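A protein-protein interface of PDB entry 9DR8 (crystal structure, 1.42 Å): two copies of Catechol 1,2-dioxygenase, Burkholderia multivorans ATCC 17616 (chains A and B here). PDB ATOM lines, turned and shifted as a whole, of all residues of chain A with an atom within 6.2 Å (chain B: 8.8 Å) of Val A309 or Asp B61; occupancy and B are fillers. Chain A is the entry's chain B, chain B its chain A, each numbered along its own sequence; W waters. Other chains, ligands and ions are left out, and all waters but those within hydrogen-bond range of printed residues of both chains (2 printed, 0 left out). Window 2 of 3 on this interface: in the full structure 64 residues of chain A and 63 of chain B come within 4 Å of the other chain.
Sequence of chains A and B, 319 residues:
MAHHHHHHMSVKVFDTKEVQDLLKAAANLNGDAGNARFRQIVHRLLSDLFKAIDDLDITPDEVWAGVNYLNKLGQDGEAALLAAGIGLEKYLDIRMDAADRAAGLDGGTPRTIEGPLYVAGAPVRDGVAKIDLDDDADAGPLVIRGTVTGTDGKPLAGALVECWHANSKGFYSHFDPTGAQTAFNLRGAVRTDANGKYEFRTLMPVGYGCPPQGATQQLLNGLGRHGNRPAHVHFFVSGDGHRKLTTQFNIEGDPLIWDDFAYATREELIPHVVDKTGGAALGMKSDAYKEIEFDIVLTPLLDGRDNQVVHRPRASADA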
ATOM      1  N   MET A  96       4.048   1.410   1.392  1.00  0.00           N
ATOM      2  CA  MET A  96       3.934   0.677   0.131  1.00  0.00           C
ATOM      3  C   MET A  96       3.318  -0.703   0.343  1.00  0.00           C
ATOM      4  O   MET A  96       2.516  -1.158  -0.480  1.00  0.00           O
ATOM      5  CB  MET A  96       5.300   0.558  -0.555  1.00  0.00           C
ATOM      6  CG  MET A  96       5.766   1.862  -1.208  1.00  0.00           C
ATOM      7  SD  MET A  96       7.248   1.688  -2.246  1.00  0.00           S
ATOM      8  CE  MET A  96       8.562   1.861  -1.047  1.00  0.00           C
ATOM      9  N   LYS A 244       9.246  -3.508 -10.556  1.00  0.00           N
ATOM     10  CA  LYS A 244      10.614  -3.630 -10.069  1.00  0.00           C
ATOM     11  C   LYS A 244      10.602  -3.892  -8.565  1.00  0.00           C
ATOM     12  O   LYS A 244      10.008  -3.126  -7.795  1.00  0.00           O
ATOM     13  CB  LYS A 244      11.391  -2.356 -10.384  1.00  0.00           C
ATOM     14  CG  LYS A 244      12.841  -2.386  -9.913  1.00  0.00           C
ATOM     15  CD  LYS A 244      13.588  -1.178 -10.416  1.00  0.00           C
ATOM     16  CE  LYS A 244      15.061  -1.223 -10.071  1.00  0.00           C
ATOM     17  NZ  LYS A 244      15.776  -0.106 -10.748  1.00  0.00           N
ATOM     18  N   ASP A 306       4.141   0.758 -13.303  1.00  0.00           N
ATOM     19  CA  ASP A 306       4.686   0.433 -11.989  1.00  0.00           C
ATOM     20  C   ASP A 306       4.523   1.648 -11.082  1.00  0.00           C
ATOM     21  O   ASP A 306       5.215   2.656 -11.247  1.00  0.00           O
ATOM     22  CB  ASP A 306       6.152   0.059 -12.161  1.00  0.00           C
ATOM     23  CG  ASP A 306       6.789  -0.430 -10.891  1.00  0.00           C
ATOM     24  OD1 ASP A 306       6.198  -0.268  -9.800  1.00  0.00           O
ATOM     25  OD2 ASP A 306       7.908  -0.968 -11.004  1.00  0.00           O
ATOM     26  N   ASN A 307       3.616   1.550 -10.111  1.00  0.00           N
ATOM     27  CA  ASN A 307       3.313   2.662  -9.224  1.00  0.00           C
ATOM     28  C   ASN A 307       3.997   2.540  -7.871  1.00  0.00           C
ATOM     29  O   ASN A 307       3.619   3.245  -6.932  1.00  0.00           O
ATOM     30  CB  ASN A 307       1.800   2.826  -9.076  1.00  0.00           C
ATOM     31  CG  ASN A 307       1.159   3.343 -10.344  1.00  0.00           C
ATOM     32  OD1 ASN A 307       0.299   2.690 -10.936  1.00  0.00           O
ATOM     33  ND2 ASN A 307       1.598   4.514 -10.787  1.00  0.00           N
ATOM     34  N   GLN A 308       5.005   1.674  -7.752  1.00  0.00           N
ATOM     35  CA  GLN A 308       5.830   1.640  -6.552  1.00  0.00           C
ATOM     36  C   GLN A 308       7.321   1.789  -6.826  1.00  0.00           C
ATOM     37  O   GLN A 308       8.098   1.870  -5.871  1.00  0.00           O
ATOM     38  CB  GLN A 308       5.548   0.391  -5.699  1.00  0.00           C
ATOM     39  CG  GLN A 308       5.712  -0.962  -6.403  1.00  0.00           C
ATOM     40  CD  GLN A 308       7.142  -1.454  -6.454  1.00  0.00           C
ATOM     41  OE1 GLN A 308       7.741  -1.796  -5.427  1.00  0.00           O
ATOM     42  NE2 GLN A 308       7.705  -1.484  -7.653  1.00  0.00           N
ATOM     43  N   VAL A 309       7.743   1.843  -8.090  1.00  0.00           N
ATOM     44  CA  VAL A 309       9.150   2.075  -8.384  1.00  0.00           C
ATOM     45  C   VAL A 309       9.549   3.461  -7.887  1.00  0.00           C
ATOM     46  O   VAL A 309       8.763   4.415  -7.945  1.00  0.00           O
ATOM     47  CB  VAL A 309       9.420   1.893  -9.888  1.00  0.00           C
ATOM     48  CG1 VAL A 309       8.705   2.973 -10.709  1.00  0.00           C
ATOM     49  CG2 VAL A 309      10.925   1.873 -10.158  1.00  0.00           C
ATOM     50  N   VAL A 310      10.772   3.570  -7.367  1.00  0.00           N
ATOM     51  CA  VAL A 310      11.246   4.768  -6.685  1.00  0.00           C
ATOM     52  C   VAL A 310      12.397   5.377  -7.471  1.00  0.00           C
ATOM     53  O   VAL A 310      13.367   4.684  -7.806  1.00  0.00           O
ATOM     54  CB  VAL A 310      11.689   4.459  -5.244  1.00  0.00           C
ATOM     55  CG1 VAL A 310      12.373   5.683  -4.619  1.00  0.00           C
ATOM     56  CG2 VAL A 310      10.490   4.043  -4.416  1.00  0.00           C
ATOM     57  N   HIS A 311      12.283   6.674  -7.753  1.00  0.00           N
ATOM     58  CA  HIS A 311      13.363   7.469  -8.308  1.00  0.00           C
ATOM     59  C   HIS A 311      13.983   8.278  -7.180  1.00  0.00           C
ATOM     60  O   HIS A 311      13.287   9.046  -6.506  1.00  0.00           O
ATOM     61  CB  HIS A 311      12.850   8.441  -9.364  1.00  0.00           C
ATOM     62  CG  HIS A 311      13.909   9.368  -9.863  1.00  0.00           C
ATOM     63  ND1 HIS A 311      14.976   8.931 -10.620  1.00  0.00           N
ATOM     64  CD2 HIS A 311      14.103  10.694  -9.669  1.00  0.00           C
ATOM     65  CE1 HIS A 311      15.759   9.955 -10.904  1.00  0.00           C
ATOM     66  NE2 HIS A 311      15.256  11.036 -10.335  1.00  0.00           N
ATOM     67  N   ARG A 312      15.276   8.088  -6.971  1.00  0.00           N
ATOM     68  CA  ARG A 312      16.035   8.854  -5.999  1.00  0.00           C
ATOM     69  C   ARG A 312      17.442   9.007  -6.538  1.00  0.00           C
ATOM     70  O   ARG A 312      17.872   8.221  -7.392  1.00  0.00           O
ATOM     71  CB  ARG A 312      16.063   8.159  -4.630  1.00  0.00           C
ATOM     72  CG  ARG A 312      16.683   6.775  -4.657  1.00  0.00           C
ATOM     73  CD  ARG A 312      16.508   6.031  -3.340  1.00  0.00           C
ATOM     74  NE  ARG A 312      17.458   6.449  -2.313  1.00  0.00           N
ATOM     75  CZ  ARG A 312      17.641   5.804  -1.168  1.00  0.00           C
ATOM     76  NH1 ARG A 312      16.929   4.729  -0.857  1.00  0.00           N
ATOM     77  NH2 ARG A 312      18.573   6.230  -0.326  1.00  0.00           N
ATOM     78  N   ASP B  57      -0.182  11.947   1.685  1.00  0.00           N
ATOM     79  CA  ASP B  57       0.261  10.901   0.767  1.00  0.00           C
ATOM     80  C   ASP B  57       1.551  11.314   0.059  1.00  0.00           C
ATOM     81  O   ASP B  57       1.666  11.282  -1.168  1.00  0.00           O
ATOM     82  CB  ASP B  57      -0.827  10.518  -0.235  1.00  0.00           C
ATOM     83  CG  ASP B  57      -0.540   9.196  -0.922  1.00  0.00           C
ATOM     84  OD1 ASP B  57       0.233   8.380  -0.370  1.00  0.00           O
ATOM     85  OD2 ASP B  57      -1.089   8.974  -2.017  1.00  0.00           O
ATOM     86  N   ILE B  58       2.538  11.712   0.855  1.00  0.00           N
ATOM     87  CA  ILE B  58       3.825  12.103   0.294  1.00  0.00           C
ATOM     88  C   ILE B  58       4.508  10.841  -0.225  1.00  0.00           C
ATOM     89  O   ILE B  58       4.678   9.860   0.508  1.00  0.00           O
ATOM     90  CB  ILE B  58       4.669  12.845   1.337  1.00  0.00           C
ATOM     91  CG1 ILE B  58       3.900  14.060   1.877  1.00  0.00           C
ATOM     92  CG2 ILE B  58       5.975  13.327   0.733  1.00  0.00           C
ATOM     93  CD1 ILE B  58       4.695  14.921   2.862  1.00  0.00           C
ATOM     94  N   THR B  59       4.876  10.845  -1.503  1.00  0.00           N
ATOM     95  CA  THR B  59       5.394   9.646  -2.139  1.00  0.00           C
ATOM     96  C   THR B  59       6.863   9.434  -1.789  1.00  0.00           C
ATOM     97  O   THR B  59       7.564  10.372  -1.397  1.00  0.00           O
ATOM     98  CB  THR B  59       5.286   9.766  -3.653  1.00  0.00           C
ATOM     99  OG1 THR B  59       6.189  10.773  -4.106  1.00  0.00           O
ATOM    100  CG2 THR B  59       3.870  10.113  -4.085  1.00  0.00           C
ATOM    101  N   PRO B  60       7.368   8.209  -1.950  1.00  0.00           N
ATOM    102  CA  PRO B  60       8.811   8.013  -1.791  1.00  0.00           C
ATOM    103  C   PRO B  60       9.630   8.947  -2.663  1.00  0.00           C
ATOM    104  O   PRO B  60      10.639   9.482  -2.192  1.00  0.00           O
ATOM    105  CB  PRO B  60       9.000   6.537  -2.152  1.00  0.00           C
ATOM    106  CG  PRO B  60       7.679   5.905  -1.737  1.00  0.00           C
ATOM    107  CD  PRO B  60       6.650   6.927  -2.114  1.00  0.00           C
ATOM    108  N   ASP B  61       9.244   9.155  -3.927  1.00  0.00           N
ATOM    109  CA  ASP B  61      10.006  10.075  -4.767  1.00  0.00           C
ATOM    110  C   ASP B  61      10.084  11.456  -4.135  1.00  0.00           C
ATOM    111  O   ASP B  61      11.149  12.089  -4.134  1.00  0.00           O
ATOM    112  CB  ASP B  61       9.388  10.192  -6.161  1.00  0.00           C
ATOM    113  CG  ASP B  61       9.641   8.968  -7.030  1.00  0.00           C
ATOM    114  OD1 ASP B  61      10.018   7.904  -6.495  1.00  0.00           O
ATOM    115  OD2 ASP B  61       9.445   9.077  -8.260  1.00  0.00           O
ATOM    116  N   GLU B  62       8.962  11.944  -3.601  1.00  0.00           N
ATOM    117  CA  GLU B  62       8.960  13.250  -2.950  1.00  0.00           C
ATOM    118  C   GLU B  62       9.865  13.248  -1.722  1.00  0.00           C
ATOM    119  O   GLU B  62      10.655  14.175  -1.523  1.00  0.00           O
ATOM    120  CB  GLU B  62       7.528  13.676  -2.585  1.00  0.00           C
ATOM    121  CG  GLU B  62       6.697  14.142  -3.778  1.00  0.00           C
ATOM    122  CD  GLU B  62       5.199  14.254  -3.498  1.00  0.00           C
ATOM    123  OE1 GLU B  62       4.689  13.554  -2.604  1.00  0.00           O
ATOM    124  OE2 GLU B  62       4.522  15.039  -4.202  1.00  0.00           O
ATOM    125  N   VAL B  63       9.769  12.205  -0.888  1.00  0.00           N
ATOM    126  CA  VAL B  63      10.605  12.127   0.310  1.00  0.00           C
ATOM    127  C   VAL B  63      12.078  12.146  -0.065  1.00  0.00           C
ATOM    128  O   VAL B  63      12.879  12.872   0.539  1.00  0.00           O
ATOM    129  CB  VAL B  63      10.239  10.890   1.151  1.00  0.00           C
ATOM    130  CG1 VAL B  63      11.242  10.691   2.268  1.00  0.00           C
ATOM    131  CG2 VAL B  63       8.830  11.046   1.721  1.00  0.00           C
ATOM    132  N   TRP B  64      12.471  11.331  -1.058  1.00  0.00           N
ATOM    133  CA  TRP B  64      13.889  11.281  -1.410  1.00  0.00           C
ATOM    134  C   TRP B  64      14.373  12.595  -2.009  1.00  0.00           C
ATOM    135  O   TRP B  64      15.560  12.920  -1.893  1.00  0.00           O
ATOM    136  CB  TRP B  64      14.194  10.093  -2.325  1.00  0.00           C
ATOM    137  CG  TRP B  64      14.017   8.800  -1.618  1.00  0.00           C
ATOM    138  CD1 TRP B  64      13.123   7.815  -1.919  1.00  0.00           C
ATOM    139  CD2 TRP B  64      14.731   8.354  -0.455  1.00  0.00           C
ATOM    140  NE1 TRP B  64      13.233   6.786  -1.020  1.00  0.00           N
ATOM    141  CE2 TRP B  64      14.219   7.084  -0.117  1.00  0.00           C
ATOM    142  CE3 TRP B  64      15.755   8.898   0.324  1.00  0.00           C
ATOM    143  CZ2 TRP B  64      14.687   6.356   0.968  1.00  0.00           C
ATOM    144  CZ3 TRP B  64      16.226   8.163   1.408  1.00  0.00           C
ATOM    145  CH2 TRP B  64      15.684   6.913   1.720  1.00  0.00           C
ATOM    146  N   ALA B  65      13.484  13.352  -2.652  1.00  0.00           N
ATOM    147  CA  ALA B  65      13.854  14.685  -3.112  1.00  0.00           C
ATOM    148  C   ALA B  65      14.078  15.624  -1.928  1.00  0.00           C
ATOM    149  O   ALA B  65      14.991  16.457  -1.954  1.00  0.00           O
ATOM    150  CB  ALA B  65      12.778  15.227  -4.050  1.00  0.00           C
ATOM    151  N   GLY B  66      13.274  15.475  -0.870  1.00  0.00           N
ATOM    152  CA  GLY B  66      13.504  16.237   0.348  1.00  0.00           C
ATOM    153  C   GLY B  66      14.787  15.839   1.057  1.00  0.00           C
ATOM    154  O   GLY B  66      15.518  16.696   1.566  1.00  0.00           O
ATOM    155  N   VAL B  67      15.085  14.534   1.084  1.00  0.00           N
ATOM    156  CA  VAL B  67      16.354  14.056   1.635  1.00  0.00           C
ATOM    157  C   VAL B  67      17.527  14.636   0.852  1.00  0.00           C
ATOM    158  O   VAL B  67      18.516  15.108   1.433  1.00  0.00           O
ATOM    159  CB  VAL B  67      16.369  12.513   1.645  1.00  0.00           C
ATOM    160  CG1 VAL B  67      17.763  11.966   1.960  1.00  0.00           C
ATOM    161  CG2 VAL B  67      15.356  11.991   2.641  1.00  0.00           C
ATOM    162  N   ASN B  68      17.428  14.622  -0.478  1.00  0.00           N
ATOM    163  CA  ASN B  68      18.493  15.168  -1.309  1.00  0.00           C
ATOM    164  C   ASN B  68      18.650  16.657  -1.061  1.00  0.00           C
ATOM    165  O   ASN B  68      19.768  17.189  -1.073  1.00  0.00           O
ATOM    166  CB  ASN B  68      18.165  14.911  -2.779  1.00  0.00           C
ATOM    167  CG  ASN B  68      19.276  15.331  -3.708  1.00  0.00           C
ATOM    168  OD1 ASN B  68      20.377  14.801  -3.649  1.00  0.00           O
ATOM    169  ND2 ASN B  68      18.987  16.282  -4.584  1.00  0.00           N
HETATM  170  O   HOH W   1      13.181  11.658  -5.842  1.00  0.00           O
HETATM  171  O   HOH W   2       9.235   6.713  -9.493  1.00  0.00           O
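N of His A311 lies within hydrogen-bond range of OD1 of Asp B61.
OG1 of Thr B59 sits close to N of Asp B61 (3.5 Å).
The backbone NH of Val A309 lies within hydrogen-bond range of the side-chain carboxylate of Asp A306 (3.1 Å).
Among the printed residues, merely in contact across the chains: Arg A312 with Trp B64, Val A310 with Asp B61, Val A310 with Trp B64, Val A310 with Pro B60 and Val A309 with Asp B61.
No residue of chain B comes within 4 Å of Gln A308.
Printed residues of chain B within 4 Å of Val A309: Asp B61 (3.98 Å).
Val A310 touches just these residues of chain B: Pro B60 (3.7 Å), Asp B61 (3.4 Å) and Trp B64 (3.5 Å).
Of the printed residues of chain B, Arg A312 touches Trp B64.
Printed residues of chain A within 4 Å of Pro B60: Val A310 (3.7 Å).
Of the printed residues of chain A, Trp B64 touches Val A310 (3.5 Å) and Arg A312 (3.3 Å).
Ala B65 touches none of the printed residues of chain A.
The nearest printed residue of chain A that does not touch Asp B61 is Arg A312 (5.3 Å).
Printed residues of chain B that touch a printed residue of chain A: Pro B60, Asp B61 and Trp B64.
Along chain B the printed residues that touch a printed residue of chain A span positions 60 to 64.
Of the 9 printed residues of chain A, 4 touch a printed residue of chain B.
Hydrophobic or aromatic side chains of chain A that line the printed part of chain B: Val A310 and His A311.
Along chain A the printed residues that touch a printed residue of chain B span positions 309 to 312.
No position is printed for both chains.
Water W2 lies within hydrogen-bond range of OD2 of Asp B61 (2.7 Å) and O of Val A309 (2.8 Å).
Water W1 lies within hydrogen-bond range of the backbone carbonyl oxygen (O) of Asp B61 (2.7 Å) and the backbone carbonyl oxygen (O) of His A311 (2.7 Å).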
